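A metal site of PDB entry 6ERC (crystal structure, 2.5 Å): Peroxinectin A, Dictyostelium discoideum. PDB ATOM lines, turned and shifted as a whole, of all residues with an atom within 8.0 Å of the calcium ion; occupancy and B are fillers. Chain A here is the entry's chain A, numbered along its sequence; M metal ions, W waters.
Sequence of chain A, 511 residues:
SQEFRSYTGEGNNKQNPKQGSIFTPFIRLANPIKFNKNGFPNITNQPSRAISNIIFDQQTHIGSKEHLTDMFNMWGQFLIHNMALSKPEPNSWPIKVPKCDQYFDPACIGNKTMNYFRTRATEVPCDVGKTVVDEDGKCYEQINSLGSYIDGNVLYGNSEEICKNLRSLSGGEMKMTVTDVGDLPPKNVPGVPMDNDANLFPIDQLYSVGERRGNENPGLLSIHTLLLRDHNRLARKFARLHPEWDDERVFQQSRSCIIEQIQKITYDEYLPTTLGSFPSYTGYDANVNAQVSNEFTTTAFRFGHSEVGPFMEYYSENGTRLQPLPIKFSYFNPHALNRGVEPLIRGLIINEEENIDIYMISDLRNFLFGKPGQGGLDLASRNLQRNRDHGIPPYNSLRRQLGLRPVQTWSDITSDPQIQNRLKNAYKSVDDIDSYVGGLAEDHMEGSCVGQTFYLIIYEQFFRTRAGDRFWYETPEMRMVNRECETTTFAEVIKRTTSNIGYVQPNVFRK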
ATOM      1  N   PHE A  56     -10.748  -9.006   6.639  1.00  0.00           N
ATOM      2  CA  PHE A  56     -10.316  -8.940   8.036  1.00  0.00           C
ATOM      3  C   PHE A  56     -10.243  -7.533   8.607  1.00  0.00           C
ATOM      4  O   PHE A  56     -10.090  -7.394   9.820  1.00  0.00           O
ATOM      5  CB  PHE A  56      -8.967  -9.630   8.181  1.00  0.00           C
ATOM      6  CG  PHE A  56      -9.031 -11.128   8.066  1.00  0.00           C
ATOM      7  CD1 PHE A  56      -9.219 -11.920   9.184  1.00  0.00           C
ATOM      8  CD2 PHE A  56      -8.933 -11.740   6.832  1.00  0.00           C
ATOM      9  CE1 PHE A  56      -9.292 -13.294   9.075  1.00  0.00           C
ATOM     10  CE2 PHE A  56      -9.007 -13.120   6.710  1.00  0.00           C
ATOM     11  CZ  PHE A  56      -9.185 -13.895   7.843  1.00  0.00           C
ATOM     12  N   GLN A  58     -10.743  -4.265  10.477  1.00  0.00           N
ATOM     13  CA  GLN A  58     -11.575  -3.945  11.635  1.00  0.00           C
ATOM     14  C   GLN A  58     -11.373  -2.476  11.986  1.00  0.00           C
ATOM     15  O   GLN A  58     -10.234  -2.006  12.059  1.00  0.00           O
ATOM     16  CB  GLN A  58     -11.225  -4.831  12.822  1.00  0.00           C
ATOM     17  CG  GLN A  58     -12.214  -4.756  13.973  1.00  0.00           C
ATOM     18  CD  GLN A  58     -12.011  -5.856  14.986  1.00  0.00           C
ATOM     19  OE1 GLN A  58     -11.260  -6.802  14.752  1.00  0.00           O
ATOM     20  NE2 GLN A  58     -12.677  -5.745  16.127  1.00  0.00           N
ATOM     21  N   THR A  60     -13.867  -0.910  14.444  1.00  0.00           N
ATOM     22  CA  THR A  60     -14.547  -0.627  15.703  1.00  0.00           C
ATOM     23  C   THR A  60     -14.450  -1.832  16.617  1.00  0.00           C
ATOM     24  O   THR A  60     -14.072  -2.940  16.208  1.00  0.00           O
ATOM     25  CB  THR A  60     -16.021  -0.290  15.467  1.00  0.00           C
ATOM     26  OG1 THR A  60     -16.733  -1.473  15.086  1.00  0.00           O
ATOM     27  CG2 THR A  60     -16.184   0.775  14.379  1.00  0.00           C
ATOM     28  N   ILE A  62     -16.091  -4.777  18.654  1.00  0.00           N
ATOM     29  CA  ILE A  62     -17.283  -5.615  18.627  1.00  0.00           C
ATOM     30  C   ILE A  62     -17.504  -6.154  20.032  1.00  0.00           C
ATOM     31  O   ILE A  62     -18.536  -5.867  20.665  1.00  0.00           O
ATOM     32  CB  ILE A  62     -17.156  -6.753  17.600  1.00  0.00           C
ATOM     33  CG1 ILE A  62     -17.139  -6.198  16.178  1.00  0.00           C
ATOM     34  CG2 ILE A  62     -18.316  -7.747  17.745  1.00  0.00           C
ATOM     35  CD1 ILE A  62     -15.779  -5.693  15.710  1.00  0.00           C
ATOM     36  N   GLY A  63     -16.552  -6.924  20.537  1.00  0.00           N
ATOM     37  CA  GLY A  63     -16.658  -7.501  21.868  1.00  0.00           C
ATOM     38  C   GLY A  63     -17.259  -8.884  21.852  1.00  0.00           C
ATOM     39  O   GLY A  63     -18.280  -9.118  21.204  1.00  0.00           O
ATOM     40  N   SER A  64     -16.637  -9.809  22.581  1.00  0.00           N
ATOM     41  CA  SER A  64     -17.065 -11.204  22.590  1.00  0.00           C
ATOM     42  C   SER A  64     -18.544 -11.313  22.903  1.00  0.00           C
ATOM     43  O   SER A  64     -19.017 -10.831  23.929  1.00  0.00           O
ATOM     44  CB  SER A  64     -16.239 -11.989  23.607  1.00  0.00           C
ATOM     45  OG  SER A  64     -16.679 -13.327  23.700  1.00  0.00           O
ATOM     46  N   PHE A 303      -8.430 -19.301  15.238  1.00  0.00           N
ATOM     47  CA  PHE A 303      -9.502 -18.351  15.525  1.00  0.00           C
ATOM     48  C   PHE A 303      -9.107 -17.327  16.577  1.00  0.00           C
ATOM     49  O   PHE A 303      -9.709 -16.248  16.639  1.00  0.00           O
ATOM     50  CB  PHE A 303     -10.750 -19.104  15.979  1.00  0.00           C
ATOM     51  CG  PHE A 303     -10.635 -19.714  17.350  1.00  0.00           C
ATOM     52  CD1 PHE A 303     -10.960 -18.987  18.482  1.00  0.00           C
ATOM     53  CD2 PHE A 303     -10.195 -21.017  17.513  1.00  0.00           C
ATOM     54  CE1 PHE A 303     -10.856 -19.543  19.744  1.00  0.00           C
ATOM     55  CE2 PHE A 303     -10.078 -21.583  18.778  1.00  0.00           C
ATOM     56  CZ  PHE A 303     -10.412 -20.839  19.886  1.00  0.00           C
ATOM     57  N   GLY A 304      -8.125 -17.645  17.430  1.00  0.00           N
ATOM     58  CA  GLY A 304      -7.799 -16.759  18.534  1.00  0.00           C
ATOM     59  C   GLY A 304      -7.336 -15.393  18.089  1.00  0.00           C
ATOM     60  O   GLY A 304      -7.467 -14.416  18.824  1.00  0.00           O
ATOM     61  N   HIS A 305      -6.782 -15.293  16.878  1.00  0.00           N
ATOM     62  CA  HIS A 305      -6.336 -13.990  16.397  1.00  0.00           C
ATOM     63  C   HIS A 305      -7.509 -13.030  16.219  1.00  0.00           C
ATOM     64  O   HIS A 305      -7.342 -11.813  16.356  1.00  0.00           O
ATOM     65  CB  HIS A 305      -5.567 -14.178  15.099  1.00  0.00           C
ATOM     66  CG  HIS A 305      -4.424 -15.138  15.231  1.00  0.00           C
ATOM     67  ND1 HIS A 305      -4.182 -16.142  14.319  1.00  0.00           N
ATOM     68  CD2 HIS A 305      -3.466 -15.257  16.180  1.00  0.00           C
ATOM     69  CE1 HIS A 305      -3.126 -16.838  14.689  1.00  0.00           C
ATOM     70  NE2 HIS A 305      -2.663 -16.314  15.814  1.00  0.00           N
ATOM     71  N   SER A 306      -8.698 -13.559  15.916  1.00  0.00           N
ATOM     72  CA  SER A 306      -9.893 -12.736  15.866  1.00  0.00           C
ATOM     73  C   SER A 306     -10.286 -12.220  17.246  1.00  0.00           C
ATOM     74  O   SER A 306     -10.815 -11.115  17.382  1.00  0.00           O
ATOM     75  CB  SER A 306     -11.045 -13.548  15.268  1.00  0.00           C
ATOM     76  OG  SER A 306     -12.179 -12.732  15.061  1.00  0.00           O
ATOM     77  N   GLU A 307     -10.042 -13.021  18.292  1.00  0.00           N
ATOM     78  CA  GLU A 307     -10.543 -12.713  19.629  1.00  0.00           C
ATOM     79  C   GLU A 307      -9.586 -11.859  20.462  1.00  0.00           C
ATOM     80  O   GLU A 307      -9.983 -11.395  21.538  1.00  0.00           O
ATOM     81  CB  GLU A 307     -10.858 -14.016  20.387  1.00  0.00           C
ATOM     82  CG  GLU A 307      -9.669 -14.679  21.064  1.00  0.00           C
ATOM     83  CD  GLU A 307      -9.947 -16.101  21.510  1.00  0.00           C
ATOM     84  OE1 GLU A 307     -11.095 -16.398  21.918  1.00  0.00           O
ATOM     85  OE2 GLU A 307      -9.011 -16.937  21.452  1.00  0.00           O
ATOM     86  N   VAL A 308      -8.357 -11.629  19.992  1.00  0.00           N
ATOM     87  CA  VAL A 308      -7.422 -10.776  20.723  1.00  0.00           C
ATOM     88  C   VAL A 308      -7.923  -9.335  20.670  1.00  0.00           C
ATOM     89  O   VAL A 308      -8.113  -8.772  19.594  1.00  0.00           O
ATOM     90  CB  VAL A 308      -6.018 -10.897  20.117  1.00  0.00           C
ATOM     91  CG1 VAL A 308      -5.073  -9.851  20.708  1.00  0.00           C
ATOM     92  CG2 VAL A 308      -5.470 -12.290  20.332  1.00  0.00           C
ATOM     93  N   GLY A 309      -8.125  -8.744  21.839  1.00  0.00           N
ATOM     94  CA  GLY A 309      -8.466  -7.341  21.925  1.00  0.00           C
ATOM     95  C   GLY A 309      -7.260  -6.459  21.714  1.00  0.00           C
ATOM     96  O   GLY A 309      -6.102  -6.900  21.745  1.00  0.00           O
ATOM     97  N   GLU A 353     -12.762  -9.945  26.013  1.00  0.00           N
ATOM     98  CA  GLU A 353     -11.977 -10.062  24.796  1.00  0.00           C
ATOM     99  C   GLU A 353     -12.828  -9.681  23.584  1.00  0.00           C
ATOM    100  O   GLU A 353     -13.968  -9.213  23.707  1.00  0.00           O
ATOM    101  CB  GLU A 353     -11.421 -11.474  24.640  1.00  0.00           C
ATOM    102  CG  GLU A 353     -12.450 -12.528  24.283  1.00  0.00           C
ATOM    103  CD  GLU A 353     -11.819 -13.856  23.916  1.00  0.00           C
ATOM    104  OE1 GLU A 353     -10.577 -13.965  24.020  1.00  0.00           O
ATOM    105  OE2 GLU A 353     -12.557 -14.784  23.519  1.00  0.00           O
ATOM    106  N   GLU A 354     -12.269  -9.884  22.402  1.00  0.00           N
ATOM    107  CA  GLU A 354     -12.924  -9.563  21.142  1.00  0.00           C
ATOM    108  C   GLU A 354     -13.703 -10.772  20.621  1.00  0.00           C
ATOM    109  O   GLU A 354     -13.475 -11.913  21.036  1.00  0.00           O
ATOM    110  CB  GLU A 354     -11.868  -9.125  20.122  1.00  0.00           C
ATOM    111  CG  GLU A 354     -12.361  -8.240  18.994  1.00  0.00           C
ATOM    112  CD  GLU A 354     -13.038  -6.976  19.483  1.00  0.00           C
ATOM    113  OE1 GLU A 354     -12.348  -6.169  20.147  1.00  0.00           O
ATOM    114  OE2 GLU A 354     -14.246  -6.800  19.206  1.00  0.00           O
ATOM    115  N   ASN A 355     -14.637 -10.505  19.709  1.00  0.00           N
ATOM    116  CA  ASN A 355     -15.485 -11.569  19.172  1.00  0.00           C
ATOM    117  C   ASN A 355     -14.724 -12.374  18.128  1.00  0.00           C
ATOM    118  O   ASN A 355     -13.833 -11.881  17.447  1.00  0.00           O
ATOM    119  CB  ASN A 355     -16.751 -10.985  18.556  1.00  0.00           C
ATOM    120  CG  ASN A 355     -17.853 -12.017  18.407  1.00  0.00           C
ATOM    121  OD1 ASN A 355     -18.207 -12.702  19.365  1.00  0.00           O
ATOM    122  ND2 ASN A 355     -18.392 -12.125  17.208  1.00  0.00           N
ATOM    123  N   ILE A 356     -15.105 -13.650  18.010  1.00  0.00           N
ATOM    124  CA  ILE A 356     -14.505 -14.540  17.015  1.00  0.00           C
ATOM    125  C   ILE A 356     -15.339 -14.410  15.736  1.00  0.00           C
ATOM    126  O   ILE A 356     -16.462 -14.919  15.658  1.00  0.00           O
ATOM    127  CB  ILE A 356     -14.449 -15.985  17.506  1.00  0.00           C
ATOM    128  CG1 ILE A 356     -13.484 -16.100  18.680  1.00  0.00           C
ATOM    129  CG2 ILE A 356     -13.995 -16.911  16.379  1.00  0.00           C
ATOM    130  CD1 ILE A 356     -13.727 -17.290  19.569  1.00  0.00           C
ATOM    131  N   ASP A 357     -14.771 -13.737  14.752  1.00  0.00           N
ATOM    132  CA  ASP A 357     -15.474 -13.398  13.520  1.00  0.00           C
ATOM    133  C   ASP A 357     -14.413 -13.088  12.473  1.00  0.00           C
ATOM    134  O   ASP A 357     -13.218 -13.322  12.693  1.00  0.00           O
ATOM    135  CB  ASP A 357     -16.433 -12.237  13.775  1.00  0.00           C
ATOM    136  CG  ASP A 357     -15.785 -11.108  14.543  1.00  0.00           C
ATOM    137  OD1 ASP A 357     -14.546 -10.991  14.467  1.00  0.00           O
ATOM    138  OD2 ASP A 357     -16.502 -10.360  15.216  1.00  0.00           O
ATOM    139  N   ILE A 358     -14.829 -12.558  11.329  1.00  0.00           N
ATOM    140  CA  ILE A 358     -13.878 -12.296  10.265  1.00  0.00           C
ATOM    141  C   ILE A 358     -12.928 -11.152  10.615  1.00  0.00           C
ATOM    142  O   ILE A 358     -11.895 -10.987   9.952  1.00  0.00           O
ATOM    143  CB  ILE A 358     -14.606 -11.985   8.946  1.00  0.00           C
ATOM    144  CG1 ILE A 358     -15.532 -10.777   9.098  1.00  0.00           C
ATOM    145  CG2 ILE A 358     -15.390 -13.213   8.485  1.00  0.00           C
ATOM    146  CD1 ILE A 358     -16.057 -10.239   7.792  1.00  0.00           C
ATOM    147  N   TYR A 359     -13.224 -10.367  11.638  1.00  0.00           N
ATOM    148  CA  TYR A 359     -12.490  -9.146  11.907  1.00  0.00           C
ATOM    149  C   TYR A 359     -11.302  -9.371  12.829  1.00  0.00           C
ATOM    150  O   TYR A 359     -11.404 -10.086  13.830  1.00  0.00           O
ATOM    151  CB  TYR A 359     -13.416  -8.103  12.515  1.00  0.00           C
ATOM    152  CG  TYR A 359     -14.660  -7.961  11.701  1.00  0.00           C
ATOM    153  CD1 TYR A 359     -14.637  -7.267  10.511  1.00  0.00           C
ATOM    154  CD2 TYR A 359     -15.843  -8.562  12.095  1.00  0.00           C
ATOM    155  CE1 TYR A 359     -15.766  -7.147   9.736  1.00  0.00           C
ATOM    156  CE2 TYR A 359     -16.979  -8.445  11.332  1.00  0.00           C
ATOM    157  CZ  TYR A 359     -16.932  -7.744  10.159  1.00  0.00           C
ATOM    158  OH  TYR A 359     -18.069  -7.618   9.398  1.00  0.00           O
ATOM    159  N   MET A 360     -10.183  -8.751  12.490  1.00  0.00           N
ATOM    160  CA  MET A 360      -8.960  -8.811  13.268  1.00  0.00           C
ATOM    161  C   MET A 360      -8.512  -7.388  13.573  1.00  0.00           C
ATOM    162  O   MET A 360      -8.504  -6.536  12.679  1.00  0.00           O
ATOM    163  CB  MET A 360      -7.870  -9.564  12.496  1.00  0.00           C
ATOM    164  CG  MET A 360      -6.558  -9.709  13.238  1.00  0.00           C
ATOM    165  SD  MET A 360      -5.411 -10.765  12.342  1.00  0.00           S
ATOM    166  CE  MET A 360      -6.315 -12.312  12.282  1.00  0.00           C
ATOM    167  N   ILE A 361      -8.150  -7.146  14.825  1.00  0.00           N
ATOM    168  CA  ILE A 361      -7.701  -5.811  15.211  1.00  0.00           C
ATOM    169  C   ILE A 361      -6.496  -5.407  14.379  1.00  0.00           C
ATOM    170  O   ILE A 361      -5.755  -6.240  13.848  1.00  0.00           O
ATOM    171  CB  ILE A 361      -7.367  -5.758  16.717  1.00  0.00           C
ATOM    172  CG1 ILE A 361      -6.361  -6.847  17.083  1.00  0.00           C
ATOM    173  CG2 ILE A 361      -8.650  -5.902  17.538  1.00  0.00           C
ATOM    174  CD1 ILE A 361      -5.811  -6.729  18.487  1.00  0.00           C
ATOM    175  N   LEU A 440     -14.484 -18.897  10.061  1.00  0.00           N
ATOM    176  CA  LEU A 440     -14.649 -17.713  10.897  1.00  0.00           C
ATOM    177  C   LEU A 440     -15.996 -17.033  10.653  1.00  0.00           C
ATOM    178  O   LEU A 440     -16.600 -16.504  11.587  1.00  0.00           O
ATOM    179  CB  LEU A 440     -13.512 -16.727  10.638  1.00  0.00           C
ATOM    180  CG  LEU A 440     -12.182 -17.120  11.270  1.00  0.00           C
ATOM    181  CD1 LEU A 440     -11.049 -16.237  10.767  1.00  0.00           C
ATOM    182  CD2 LEU A 440     -12.277 -17.036  12.779  1.00  0.00           C
HETATM  183 CA    CA M   1     -12.634 -10.566  15.795  1.00  0.00          CA
HETATM  184  O   HOH W   1     -11.346  -8.626  16.265  1.00  0.00           O
HETATM  185  O   HOH W   2     -14.300  -9.011  16.348  1.00  0.00           O
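O of Tyr 359 sits close to OE1 of Gln 58 (3.4 Å).
The backbone NH (N) of Glu 354 is in hydrogen-bond range of the backbone carbonyl oxygen (O) of Glu 307 (2.9 Å).
N of Ile 62 lies within hydrogen-bond range of OE2 of Glu 354, 2.8 Å away.
The backbone NH (N) of Gly 63 lies within hydrogen-bond range of the side-chain carboxylate (OE2) of Glu 354, 2.7 Å away.
Glu 354 touches the calcium ion.
The calcium ion is bound by OG of Ser 306 (2.3 Å), water W2 (2.3 Å), OD1 of Asp 357 (2.4 Å), O of Tyr 359 (2.4 Å), water W1 (2.4 Å), O of Asn 355 (2.4 Å) and O of Ser 306 (2.5 Å).
The calcium ion has seven donor atoms within binding distance.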
